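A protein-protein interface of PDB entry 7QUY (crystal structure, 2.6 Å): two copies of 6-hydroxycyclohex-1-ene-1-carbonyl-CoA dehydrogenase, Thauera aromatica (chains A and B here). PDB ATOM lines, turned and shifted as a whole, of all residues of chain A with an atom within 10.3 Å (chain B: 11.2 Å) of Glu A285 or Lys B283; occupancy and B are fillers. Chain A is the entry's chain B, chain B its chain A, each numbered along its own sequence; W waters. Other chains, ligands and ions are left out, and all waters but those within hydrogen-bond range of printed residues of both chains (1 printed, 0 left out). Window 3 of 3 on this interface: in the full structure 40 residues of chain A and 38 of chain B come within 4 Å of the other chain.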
ATOM      1  N   THR A 257      -4.768 -21.755   5.653  1.00  0.00           N
ATOM      2  CA  THR A 257      -5.403 -20.937   6.717  1.00  0.00           C
ATOM      3  C   THR A 257      -4.368 -20.631   7.806  1.00  0.00           C
ATOM      4  O   THR A 257      -3.541 -21.511   8.101  1.00  0.00           O
ATOM      5  CB  THR A 257      -6.603 -21.670   7.321  1.00  0.00           C
ATOM      6  OG1 THR A 257      -6.071 -22.530   8.323  1.00  0.00           O
ATOM      7  CG2 THR A 257      -7.402 -22.475   6.319  1.00  0.00           C
ATOM      8  N   GLY A 258      -4.416 -19.444   8.400  1.00  0.00           N
ATOM      9  CA  GLY A 258      -3.461 -19.035   9.448  1.00  0.00           C
ATOM     10  C   GLY A 258      -3.541 -19.956  10.645  1.00  0.00           C
ATOM     11  O   GLY A 258      -2.512 -20.148  11.292  1.00  0.00           O
ATOM     12  N   ALA A 259      -4.720 -20.493  10.955  1.00  0.00           N
ATOM     13  CA  ALA A 259      -4.914 -21.447  12.074  1.00  0.00           C
ATOM     14  C   ALA A 259      -4.012 -22.669  11.834  1.00  0.00           C
ATOM     15  O   ALA A 259      -3.206 -23.015  12.720  1.00  0.00           O
ATOM     16  CB  ALA A 259      -6.371 -21.843  12.185  1.00  0.00           C
ATOM     17  N   GLY A 260      -4.142 -23.275  10.653  1.00  0.00           N
ATOM     18  CA  GLY A 260      -3.321 -24.411  10.205  1.00  0.00           C
ATOM     19  C   GLY A 260      -1.841 -24.116  10.325  1.00  0.00           C
ATOM     20  O   GLY A 260      -1.113 -24.952  10.877  1.00  0.00           O
ATOM     21  N   GLN A 261      -1.414 -22.954   9.837  1.00  0.00           N
ATOM     22  CA  GLN A 261       0.008 -22.523   9.827  1.00  0.00           C
ATOM     23  C   GLN A 261       0.501 -22.426  11.270  1.00  0.00           C
ATOM     24  O   GLN A 261       1.560 -23.008  11.572  1.00  0.00           O
ATOM     25  CB  GLN A 261       0.151 -21.212   9.055  1.00  0.00           C
ATOM     26  CG  GLN A 261      -0.134 -21.375   7.566  1.00  0.00           C
ATOM     27  CD  GLN A 261       0.123 -20.129   6.761  1.00  0.00           C
ATOM     28  OE1 GLN A 261      -0.012 -19.000   7.238  1.00  0.00           O
ATOM     29  NE2 GLN A 261       0.494 -20.335   5.509  1.00  0.00           N
ATOM     30  N   THR A 262      -0.246 -21.742  12.135  1.00  0.00           N
ATOM     31  CA  THR A 262       0.098 -21.549  13.568  1.00  0.00           C
ATOM     32  C   THR A 262       0.262 -22.922  14.218  1.00  0.00           C
ATOM     33  O   THR A 262       1.242 -23.115  14.955  1.00  0.00           O
ATOM     34  CB  THR A 262      -0.959 -20.694  14.272  1.00  0.00           C
ATOM     35  OG1 THR A 262      -0.954 -19.431  13.616  1.00  0.00           O
ATOM     36  CG2 THR A 262      -0.685 -20.499  15.744  1.00  0.00           C
ATOM     37  N   SER A 263      -0.651 -23.842  13.918  1.00  0.00           N
ATOM     38  CA  SER A 263      -0.692 -25.210  14.483  1.00  0.00           C
ATOM     39  C   SER A 263       0.582 -25.954  14.067  1.00  0.00           C
ATOM     40  O   SER A 263       1.274 -26.471  14.962  1.00  0.00           O
ATOM     41  CB  SER A 263      -1.947 -25.935  14.029  1.00  0.00           C
ATOM     42  OG  SER A 263      -2.398 -26.841  15.005  1.00  0.00           O
ATOM     43  N   ALA A 264       0.863 -25.976  12.758  1.00  0.00           N
ATOM     44  CA  ALA A 264       1.996 -26.673  12.103  1.00  0.00           C
ATOM     45  C   ALA A 264       3.311 -26.148  12.672  1.00  0.00           C
ATOM     46  O   ALA A 264       4.153 -26.967  13.066  1.00  0.00           O
ATOM     47  CB  ALA A 264       1.957 -26.481  10.599  1.00  0.00           C
ATOM     48  N   TYR A 265       3.476 -24.825  12.730  1.00  0.00           N
ATOM     49  CA  TYR A 265       4.717 -24.185  13.235  1.00  0.00           C
ATOM     50  C   TYR A 265       4.945 -24.610  14.691  1.00  0.00           C
ATOM     51  O   TYR A 265       6.111 -24.830  15.065  1.00  0.00           O
ATOM     52  CB  TYR A 265       4.686 -22.663  13.071  1.00  0.00           C
ATOM     53  CG  TYR A 265       6.052 -22.050  13.235  1.00  0.00           C
ATOM     54  CD1 TYR A 265       6.910 -21.937  12.157  1.00  0.00           C
ATOM     55  CD2 TYR A 265       6.522 -21.667  14.477  1.00  0.00           C
ATOM     56  CE1 TYR A 265       8.184 -21.414  12.299  1.00  0.00           C
ATOM     57  CE2 TYR A 265       7.789 -21.143  14.638  1.00  0.00           C
ATOM     58  CZ  TYR A 265       8.625 -21.016  13.545  1.00  0.00           C
ATOM     59  OH  TYR A 265       9.884 -20.512  13.695  1.00  0.00           O
ATOM     60  N   GLY A 266       3.864 -24.741  15.469  1.00  0.00           N
ATOM     61  CA  GLY A 266       3.906 -25.158  16.884  1.00  0.00           C
ATOM     62  C   GLY A 266       4.424 -26.581  17.049  1.00  0.00           C
ATOM     63  O   GLY A 266       4.884 -26.922  18.166  1.00  0.00           O
ATOM     64  N   THR A 280      -2.350 -18.464   2.256  1.00  0.00           N
ATOM     65  CA  THR A 280      -3.279 -17.471   2.849  1.00  0.00           C
ATOM     66  C   THR A 280      -2.583 -16.106   2.836  1.00  0.00           C
ATOM     67  O   THR A 280      -1.330 -16.084   2.850  1.00  0.00           O
ATOM     68  CB  THR A 280      -3.707 -17.856   4.270  1.00  0.00           C
ATOM     69  OG1 THR A 280      -4.733 -16.951   4.670  1.00  0.00           O
ATOM     70  CG2 THR A 280      -2.582 -17.794   5.280  1.00  0.00           C
ATOM     71  N   ASP A 282      -3.395 -14.106   5.328  1.00  0.00           N
ATOM     72  CA  ASP A 282      -3.352 -13.941   6.811  1.00  0.00           C
ATOM     73  C   ASP A 282      -1.898 -13.947   7.300  1.00  0.00           C
ATOM     74  O   ASP A 282      -1.120 -14.819   6.856  1.00  0.00           O
ATOM     75  CB  ASP A 282      -4.125 -15.040   7.542  1.00  0.00           C
ATOM     76  CG  ASP A 282      -5.637 -14.996   7.353  1.00  0.00           C
ATOM     77  OD1 ASP A 282      -6.142 -14.043   6.712  1.00  0.00           O
ATOM     78  OD2 ASP A 282      -6.303 -15.935   7.833  1.00  0.00           O
ATOM     79  N   LYS A 283      -1.560 -13.006   8.186  1.00  0.00           N
ATOM     80  CA  LYS A 283      -0.292 -12.992   8.952  1.00  0.00           C
ATOM     81  C   LYS A 283      -0.472 -13.958  10.138  1.00  0.00           C
ATOM     82  O   LYS A 283      -1.624 -14.311  10.434  1.00  0.00           O
ATOM     83  CB  LYS A 283       0.072 -11.549   9.340  1.00  0.00           C
ATOM     84  N   VAL A 284       0.629 -14.435  10.733  1.00  0.00           N
ATOM     85  CA  VAL A 284       0.664 -15.352  11.913  1.00  0.00           C
ATOM     86  C   VAL A 284       1.784 -14.891  12.858  1.00  0.00           C
ATOM     87  O   VAL A 284       2.823 -14.386  12.381  1.00  0.00           O
ATOM     88  CB  VAL A 284       0.837 -16.833  11.504  1.00  0.00           C
ATOM     89  CG1 VAL A 284      -0.261 -17.285  10.547  1.00  0.00           C
ATOM     90  CG2 VAL A 284       2.207 -17.121  10.899  1.00  0.00           C
ATOM     91  N   GLU A 285       1.552 -15.038  14.162  1.00  0.00           N
ATOM     92  CA  GLU A 285       2.485 -14.724  15.270  1.00  0.00           C
ATOM     93  C   GLU A 285       3.273 -16.010  15.572  1.00  0.00           C
ATOM     94  O   GLU A 285       2.611 -17.000  15.945  1.00  0.00           O
ATOM     95  CB  GLU A 285       1.631 -14.226  16.447  1.00  0.00           C
ATOM     96  CG  GLU A 285       2.404 -13.798  17.690  1.00  0.00           C
ATOM     97  CD  GLU A 285       2.451 -12.293  17.906  1.00  0.00           C
ATOM     98  OE1 GLU A 285       1.403 -11.642  17.706  1.00  0.00           O
ATOM     99  OE2 GLU A 285       3.537 -11.771  18.258  1.00  0.00           O
ATOM    100  N   VAL A 286       4.601 -16.032  15.378  1.00  0.00           N
ATOM    101  CA  VAL A 286       5.453 -17.251  15.589  1.00  0.00           C
ATOM    102  C   VAL A 286       6.815 -16.857  16.176  1.00  0.00           C
ATOM    103  O   VAL A 286       7.293 -15.753  15.883  1.00  0.00           O
ATOM    104  CB  VAL A 286       5.639 -18.090  14.304  1.00  0.00           C
ATOM    105  CG1 VAL A 286       4.351 -18.768  13.878  1.00  0.00           C
ATOM    106  CG2 VAL A 286       6.205 -17.272  13.159  1.00  0.00           C
ATOM    107  N   ARG A 287       7.407 -17.745  16.982  1.00  0.00           N
ATOM    108  CA  ARG A 287       8.810 -17.614  17.445  1.00  0.00           C
ATOM    109  C   ARG A 287       9.686 -18.124  16.293  1.00  0.00           C
ATOM    110  O   ARG A 287       9.978 -19.346  16.236  1.00  0.00           O
ATOM    111  CB  ARG A 287       9.051 -18.340  18.777  1.00  0.00           C
ATOM    112  CG  ARG A 287      10.331 -17.906  19.492  1.00  0.00           C
ATOM    113  CD  ARG A 287      10.512 -18.448  20.900  1.00  0.00           C
ATOM    114  NE  ARG A 287       9.480 -17.916  21.783  1.00  0.00           N
ATOM    115  CZ  ARG A 287       8.418 -18.588  22.226  1.00  0.00           C
ATOM    116  NH1 ARG A 287       7.547 -17.975  23.010  1.00  0.00           N
ATOM    117  NH2 ARG A 287       8.222 -19.860  21.900  1.00  0.00           N
ATOM    118  N   LEU A 288      10.079 -17.213  15.401  1.00  0.00           N
ATOM    119  CA  LEU A 288      10.920 -17.514  14.211  1.00  0.00           C
ATOM    120  C   LEU A 288      12.229 -18.172  14.660  1.00  0.00           C
ATOM    121  O   LEU A 288      12.746 -18.992  13.907  1.00  0.00           O
ATOM    122  CB  LEU A 288      11.203 -16.220  13.442  1.00  0.00           C
ATOM    123  CG  LEU A 288      11.141 -16.267  11.914  1.00  0.00           C
ATOM    124  CD1 LEU A 288      12.337 -15.525  11.320  1.00  0.00           C
ATOM    125  CD2 LEU A 288      11.090 -17.687  11.365  1.00  0.00           C
ATOM    126  N   SER A 289      12.733 -17.828  15.842  1.00  0.00           N
ATOM    127  CA  SER A 289      14.050 -18.300  16.348  1.00  0.00           C
ATOM    128  C   SER A 289      13.992 -19.800  16.671  1.00  0.00           C
ATOM    129  O   SER A 289      15.069 -20.444  16.706  1.00  0.00           O
ATOM    130  CB  SER A 289      14.511 -17.501  17.543  1.00  0.00           C
ATOM    131  OG  SER A 289      13.978 -16.181  17.536  1.00  0.00           O
ATOM    132  N   ASN A 290      12.794 -20.353  16.877  1.00  0.00           N
ATOM    133  CA  ASN A 290      12.626 -21.815  17.063  1.00  0.00           C
ATOM    134  C   ASN A 290      13.354 -22.561  15.933  1.00  0.00           C
ATOM    135  O   ASN A 290      13.884 -23.654  16.199  1.00  0.00           O
ATOM    136  CB  ASN A 290      11.150 -22.199  17.169  1.00  0.00           C
ATOM    137  CG  ASN A 290      10.554 -21.877  18.524  1.00  0.00           C
ATOM    138  OD1 ASN A 290      11.266 -21.468  19.441  1.00  0.00           O
ATOM    139  ND2 ASN A 290       9.247 -22.044  18.659  1.00  0.00           N
ATOM    140  N   GLY B 256      19.303 -11.195  16.483  1.00  0.00           N
ATOM    141  CA  GLY B 256      18.682 -11.859  17.635  1.00  0.00           C
ATOM    142  C   GLY B 256      17.659 -10.940  18.276  1.00  0.00           C
ATOM    143  O   GLY B 256      17.535 -10.951  19.528  1.00  0.00           O
ATOM    144  N   THR B 257      16.951 -10.181  17.440  1.00  0.00           N
ATOM    145  CA  THR B 257      15.892  -9.215  17.833  1.00  0.00           C
ATOM    146  C   THR B 257      14.711  -9.355  16.867  1.00  0.00           C
ATOM    147  O   THR B 257      14.946  -9.588  15.674  1.00  0.00           O
ATOM    148  CB  THR B 257      16.418  -7.776  17.809  1.00  0.00           C
ATOM    149  OG1 THR B 257      16.312  -7.333  16.456  1.00  0.00           O
ATOM    150  CG2 THR B 257      17.849  -7.636  18.288  1.00  0.00           C
ATOM    151  N   GLY B 258      13.489  -9.213  17.363  1.00  0.00           N
ATOM    152  CA  GLY B 258      12.258  -9.306  16.560  1.00  0.00           C
ATOM    153  C   GLY B 258      12.263  -8.320  15.413  1.00  0.00           C
ATOM    154  O   GLY B 258      11.729  -8.652  14.343  1.00  0.00           O
ATOM    155  N   ALA B 259      12.823  -7.129  15.627  1.00  0.00           N
ATOM    156  CA  ALA B 259      12.905  -6.071  14.596  1.00  0.00           C
ATOM    157  C   ALA B 259      13.714  -6.614  13.411  1.00  0.00           C
ATOM    158  O   ALA B 259      13.202  -6.593  12.271  1.00  0.00           O
ATOM    159  CB  ALA B 259      13.520  -4.832  15.177  1.00  0.00           C
ATOM    160  N   GLY B 260      14.916  -7.115  13.690  1.00  0.00           N
ATOM    161  CA  GLY B 260      15.802  -7.750  12.698  1.00  0.00           C
ATOM    162  C   GLY B 260      15.092  -8.851  11.930  1.00  0.00           C
ATOM    163  O   GLY B 260      15.177  -8.849  10.692  1.00  0.00           O
ATOM    164  N   GLN B 261      14.402  -9.744  12.643  1.00  0.00           N
ATOM    165  CA  GLN B 261      13.690 -10.904  12.052  1.00  0.00           C
ATOM    166  C   GLN B 261      12.618 -10.388  11.092  1.00  0.00           C
ATOM    167  O   GLN B 261      12.588 -10.850   9.933  1.00  0.00           O
ATOM    168  CB  GLN B 261      13.127 -11.804  13.155  1.00  0.00           C
ATOM    169  CG  GLN B 261      14.227 -12.524  13.923  1.00  0.00           C
ATOM    170  CD  GLN B 261      13.726 -13.511  14.952  1.00  0.00           C
ATOM    171  OE1 GLN B 261      12.618 -13.414  15.495  1.00  0.00           O
ATOM    172  NE2 GLN B 261      14.571 -14.488  15.238  1.00  0.00           N
ATOM    173  N   THR B 262      11.790  -9.450  11.555  1.00  0.00           N
ATOM    174  CA  THR B 262      10.681  -8.859  10.762  1.00  0.00           C
ATOM    175  C   THR B 262      11.259  -8.230   9.487  1.00  0.00           C
ATOM    176  O   THR B 262      10.688  -8.432   8.399  1.00  0.00           O
ATOM    177  CB  THR B 262       9.893  -7.854  11.603  1.00  0.00           C
ATOM    178  OG1 THR B 262       9.372  -8.585  12.713  1.00  0.00           O
ATOM    179  CG2 THR B 262       8.757  -7.216  10.835  1.00  0.00           C
ATOM    180  N   SER B 263      12.378  -7.531   9.626  1.00  0.00           N
ATOM    181  CA  SER B 263      13.070  -6.821   8.522  1.00  0.00           C
ATOM    182  C   SER B 263      13.535  -7.845   7.483  1.00  0.00           C
ATOM    183  O   SER B 263      13.185  -7.674   6.291  1.00  0.00           O
ATOM    184  CB  SER B 263      14.223  -5.990   9.047  1.00  0.00           C
ATOM    185  OG  SER B 263      14.340  -4.787   8.317  1.00  0.00           O
ATOM    186  N   TYR B 265      12.695 -11.099   7.072  1.00  0.00           N
ATOM    187  CA  TYR B 265      11.566 -11.853   6.465  1.00  0.00           C
ATOM    188  C   TYR B 265      10.947 -11.014   5.343  1.00  0.00           C
ATOM    189  O   TYR B 265      10.555 -11.597   4.310  1.00  0.00           O
ATOM    190  CB  TYR B 265      10.514 -12.271   7.498  1.00  0.00           C
ATOM    191  CG  TYR B 265       9.594 -13.341   6.966  1.00  0.00           C
ATOM    192  CD1 TYR B 265       9.921 -14.679   7.069  1.00  0.00           C
ATOM    193  CD2 TYR B 265       8.424 -13.015   6.308  1.00  0.00           C
ATOM    194  CE1 TYR B 265       9.094 -15.667   6.561  1.00  0.00           C
ATOM    195  CE2 TYR B 265       7.586 -13.987   5.789  1.00  0.00           C
ATOM    196  CZ  TYR B 265       7.915 -15.325   5.922  1.00  0.00           C
ATOM    197  OH  TYR B 265       7.103 -16.305   5.412  1.00  0.00           O
ATOM    198  N   GLY B 278      20.327 -15.657  14.721  1.00  0.00           N
ATOM    199  CA  GLY B 278      19.996 -14.968  15.981  1.00  0.00           C
ATOM    200  C   GLY B 278      18.851 -15.643  16.702  1.00  0.00           C
ATOM    201  O   GLY B 278      17.936 -16.111  16.023  1.00  0.00           O
ATOM    202  N   PHE B 279      18.911 -15.664  18.036  1.00  0.00           N
ATOM    203  CA  PHE B 279      17.837 -16.160  18.935  1.00  0.00           C
ATOM    204  C   PHE B 279      17.203 -14.988  19.704  1.00  0.00           C
ATOM    205  O   PHE B 279      17.928 -14.213  20.351  1.00  0.00           O
ATOM    206  CB  PHE B 279      18.387 -17.202  19.913  1.00  0.00           C
ATOM    207  CG  PHE B 279      17.365 -17.678  20.909  1.00  0.00           C
ATOM    208  CD1 PHE B 279      16.443 -18.653  20.559  1.00  0.00           C
ATOM    209  CD2 PHE B 279      17.295 -17.116  22.177  1.00  0.00           C
ATOM    210  CE1 PHE B 279      15.479 -19.070  21.465  1.00  0.00           C
ATOM    211  CE2 PHE B 279      16.333 -17.536  23.082  1.00  0.00           C
ATOM    212  CZ  PHE B 279      15.422 -18.503  22.719  1.00  0.00           C
ATOM    213  N   THR B 280      15.878 -14.876  19.639  1.00  0.00           N
ATOM    214  CA  THR B 280      15.053 -14.050  20.559  1.00  0.00           C
ATOM    215  C   THR B 280      13.869 -14.898  21.026  1.00  0.00           C
ATOM    216  O   THR B 280      13.487 -15.824  20.289  1.00  0.00           O
ATOM    217  CB  THR B 280      14.580 -12.739  19.917  1.00  0.00           C
ATOM    218  OG1 THR B 280      13.947 -11.939  20.915  1.00  0.00           O
ATOM    219  CG2 THR B 280      13.599 -12.939  18.786  1.00  0.00           C
ATOM    220  N   MET B 281      13.319 -14.576  22.197  1.00  0.00           N
ATOM    221  CA  MET B 281      12.076 -15.200  22.714  1.00  0.00           C
ATOM    222  C   MET B 281      10.876 -14.458  22.121  1.00  0.00           C
ATOM    223  O   MET B 281       9.804 -15.081  22.079  1.00  0.00           O
ATOM    224  CB  MET B 281      12.016 -15.184  24.246  1.00  0.00           C
ATOM    225  CG  MET B 281      12.956 -16.190  24.919  1.00  0.00           C
ATOM    226  SD  MET B 281      12.573 -17.944  24.587  1.00  0.00           S
ATOM    227  CE  MET B 281      10.835 -18.039  25.022  1.00  0.00           C
ATOM    228  N   ASP B 282      11.080 -13.236  21.612  1.00  0.00           N
ATOM    229  CA  ASP B 282      10.019 -12.411  20.968  1.00  0.00           C
ATOM    230  C   ASP B 282       9.337 -13.199  19.844  1.00  0.00           C
ATOM    231  O   ASP B 282      10.058 -13.816  19.016  1.00  0.00           O
ATOM    232  CB  ASP B 282      10.571 -11.119  20.354  1.00  0.00           C
ATOM    233  CG  ASP B 282      11.069 -10.089  21.349  1.00  0.00           C
ATOM    234  OD1 ASP B 282      10.910 -10.318  22.576  1.00  0.00           O
ATOM    235  OD2 ASP B 282      11.615  -9.068  20.883  1.00  0.00           O
ATOM    236  N   LYS B 283       8.002 -13.167  19.806  1.00  0.00           N
ATOM    237  CA  LYS B 283       7.209 -13.647  18.645  1.00  0.00           C
ATOM    238  C   LYS B 283       7.207 -12.503  17.614  1.00  0.00           C
ATOM    239  O   LYS B 283       7.512 -11.366  18.011  1.00  0.00           O
ATOM    240  CB  LYS B 283       5.829 -14.129  19.111  1.00  0.00           C
ATOM    241  N   VAL B 284       6.983 -12.815  16.330  1.00  0.00           N
ATOM    242  CA  VAL B 284       6.917 -11.838  15.194  1.00  0.00           C
ATOM    243  C   VAL B 284       5.747 -12.219  14.273  1.00  0.00           C
ATOM    244  O   VAL B 284       5.446 -13.431  14.151  1.00  0.00           O
ATOM    245  CB  VAL B 284       8.245 -11.759  14.413  1.00  0.00           C
ATOM    246  CG1 VAL B 284       9.417 -11.420  15.321  1.00  0.00           C
ATOM    247  CG2 VAL B 284       8.550 -13.025  13.620  1.00  0.00           C
ATOM    248  N   GLU B 285       5.097 -11.218  13.674  1.00  0.00           N
ATOM    249  CA  GLU B 285       3.935 -11.384  12.766  1.00  0.00           C
ATOM    250  C   GLU B 285       4.494 -11.441  11.338  1.00  0.00           C
ATOM    251  O   GLU B 285       5.153 -10.456  10.941  1.00  0.00           O
ATOM    252  CB  GLU B 285       2.915 -10.259  12.992  1.00  0.00           C
ATOM    253  N   VAL B 286       4.294 -12.552  10.611  1.00  0.00           N
ATOM    254  CA  VAL B 286       4.820 -12.724   9.218  1.00  0.00           C
ATOM    255  C   VAL B 286       3.784 -13.438   8.342  1.00  0.00           C
ATOM    256  O   VAL B 286       3.008 -14.245   8.865  1.00  0.00           O
ATOM    257  CB  VAL B 286       6.166 -13.470   9.200  1.00  0.00           C
ATOM    258  CG1 VAL B 286       7.279 -12.647   9.814  1.00  0.00           C
ATOM    259  CG2 VAL B 286       6.087 -14.824   9.877  1.00  0.00           C
ATOM    260  N   ARG B 287       3.775 -13.124   7.044  1.00  0.00           N
ATOM    261  CA  ARG B 287       2.988 -13.872   6.028  1.00  0.00           C
ATOM    262  C   ARG B 287       3.788 -15.141   5.698  1.00  0.00           C
ATOM    263  O   ARG B 287       4.653 -15.102   4.793  1.00  0.00           O
ATOM    264  CB  ARG B 287       2.683 -12.988   4.813  1.00  0.00           C
ATOM    265  CG  ARG B 287       1.524 -13.476   3.948  1.00  0.00           C
ATOM    266  CD  ARG B 287       1.085 -12.523   2.833  1.00  0.00           C
ATOM    267  NE  ARG B 287       1.402 -11.106   3.036  1.00  0.00           N
ATOM    268  CZ  ARG B 287       0.716 -10.246   3.800  1.00  0.00           C
ATOM    269  NH1 ARG B 287      -0.357 -10.631   4.469  1.00  0.00           N
ATOM    270  NH2 ARG B 287       1.121  -8.993   3.908  1.00  0.00           N
ATOM    271  N   LEU B 288       3.525 -16.219   6.440  1.00  0.00           N
ATOM    272  CA  LEU B 288       4.251 -17.509   6.322  1.00  0.00           C
ATOM    273  C   LEU B 288       4.134 -18.026   4.884  1.00  0.00           C
ATOM    274  O   LEU B 288       5.067 -18.688   4.431  1.00  0.00           O
ATOM    275  CB  LEU B 288       3.657 -18.530   7.303  1.00  0.00           C
ATOM    276  CG  LEU B 288       4.624 -19.471   8.034  1.00  0.00           C
ATOM    277  CD1 LEU B 288       4.139 -20.906   7.947  1.00  0.00           C
ATOM    278  CD2 LEU B 288       6.041 -19.403   7.498  1.00  0.00           C
ATOM    279  N   SER B 289       3.017 -17.748   4.202  1.00  0.00           N
ATOM    280  CA  SER B 289       2.732 -18.308   2.856  1.00  0.00           C
ATOM    281  C   SER B 289       3.656 -17.679   1.811  1.00  0.00           C
ATOM    282  O   SER B 289       3.832 -18.306   0.740  1.00  0.00           O
ATOM    283  CB  SER B 289       1.291 -18.170   2.487  1.00  0.00           C
ATOM    284  OG  SER B 289       0.478 -18.455   3.612  1.00  0.00           O
HETATM  285  O   HOH W   1       4.974  -9.715  19.098  1.00  0.00           O
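The side-chain hydroxyl (OG1) of Thr B280 sits at hydrogen-bond distance from the backbone NH (N) of Asp B282 (3.2 Å). The side-chain hydroxyl (OH) of Tyr B265 sits close to the backbone carbonyl oxygen (O) of Leu B288 (3.3 Å). OG1 of Thr A280 sits at hydrogen-bond distance from N of Asp A282, 3.2 Å away. The backbone carbonyl oxygen (O) of Leu A288 sits close to the side-chain hydroxyl (OH) of Tyr A265, at 3.2 Å. OH of Tyr A265 sits at hydrogen-bond distance from O of Arg A287, 2.8 Å away.
The side-chain hydroxyl (OG) of Ser B289 is in hydrogen-bond range of the side-chain amide nitrogen (NE2) of Gln A261 (2.7 Å). The backbone NH (N) of Val B284 lies within hydrogen-bond range of the backbone carbonyl oxygen (O) of Val A286, 3.0 Å away. The backbone carbonyl oxygen of Thr A280 lies within hydrogen-bond range of the side-chain hydroxyl of Ser B289, at 3.1 Å. The backbone carbonyl oxygen (O) of Met B281 is in hydrogen-bond range of the guanidinium group (NE) of Arg A287, 2.9 Å away. The backbone carbonyl oxygen (O) of Val A284 sits close to the backbone carbonyl oxygen (O) of Val B284 (3.3 Å). The side-chain amide nitrogen (NE2) of Gln B261 sits at hydrogen-bond distance from the side-chain hydroxyl (OG) of Ser A289 (2.9 Å). The backbone carbonyl oxygen of Thr B280 sits at hydrogen-bond distance from the side-chain hydroxyl of Ser A289 (2.8 Å). The backbone carbonyl oxygen (O) of Val A284 sits at hydrogen-bond distance from the backbone NH (N) of Val B286 (2.9 Å).
Of the 20 printed residues of chain A, 9 touch a printed residue of chain B. Among the printed residues, 18 pairs touch across the chains. Among the printed residues, no Asp or Glu carboxylate lies within 4 Å of a Lys or Arg side-chain nitrogen of the other chain.
Water W1 lies within hydrogen-bond range of OE2 of Glu A285 and O of Lys B283.
Val A284 touches its own counterpart, Val B284. Val A284 touches Glu B285, and with the chains exchanged Glu A285 touches Val B284. Glu A285 touches Lys B283, but with the chains exchanged Lys A283 does not touch Glu B285 (4.8 Å). Arg A287 touches Thr B280, but with the chains exchanged Thr A280 does not touch Arg B287 (4.02 Å). Positions printed for both chains: 257, 258, 259, 260, 261, 262, 263, 265, 280, 282, 283, 284, 285, 286, 287, 288 and 289.
Printed residues of chain B within 4 Å of Gln A261: Leu B288 (3.7 Å) and Ser B289 (2.7 Å). No residue of chain B comes within 4 Å of Thr A262. Ser A263 touches none of the printed residues of chain B. Gly A266 touches none of the printed residues of chain B. Lys A283 touches just one residue of chain B: Val B286 (3.5 Å). Val A284 touches just these residues of chain B: Val B284 (3.3 Å), Glu B285 (3.2 Å) and Val B286 (2.9 Å). Glu A285 touches just these residues of chain B: Lys B283 (3.4 Å) and Val B284 (3.4 Å). Printed residues of chain B within 4 Å of Val A286: Lys B283 and Val B284. Of chain A, only Glu A285 and Val A286 come within 4 Å of Lys B283. Of chain A, only Val A284, Glu A285 and Val A286 come within 4 Å of Val B284. Printed residues of chain A within 4 Å of Leu B288: Gln A261. The nearest residue of chain B that does not touch Glu A285 is Glu B285 (4.4 Å). The nearest printed residue of chain A that does not touch Glu B285 is Glu A285 (4.4 Å).
Gln A261 touches Leu B288. Val B286 touches Lys A283 (O to CA, 3.5 Å). O of Val A284 touches CA of Glu B285 (3.2 Å). Glu A285 touches Lys B283 (OE2 to CB, 3.4 Å). Glu A285 touches Val B284 (CA to O, 3.4 Å). CA of Lys B283 touches O of Val A286, at 3.5 Å. O of Thr B280 touches CG of Arg A287 (3.9 Å). Gln B261 touches Leu A288. CB of Ser A289 touches O of Gly B278, at 3.997 Å. Ser A289 touches Phe B279.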
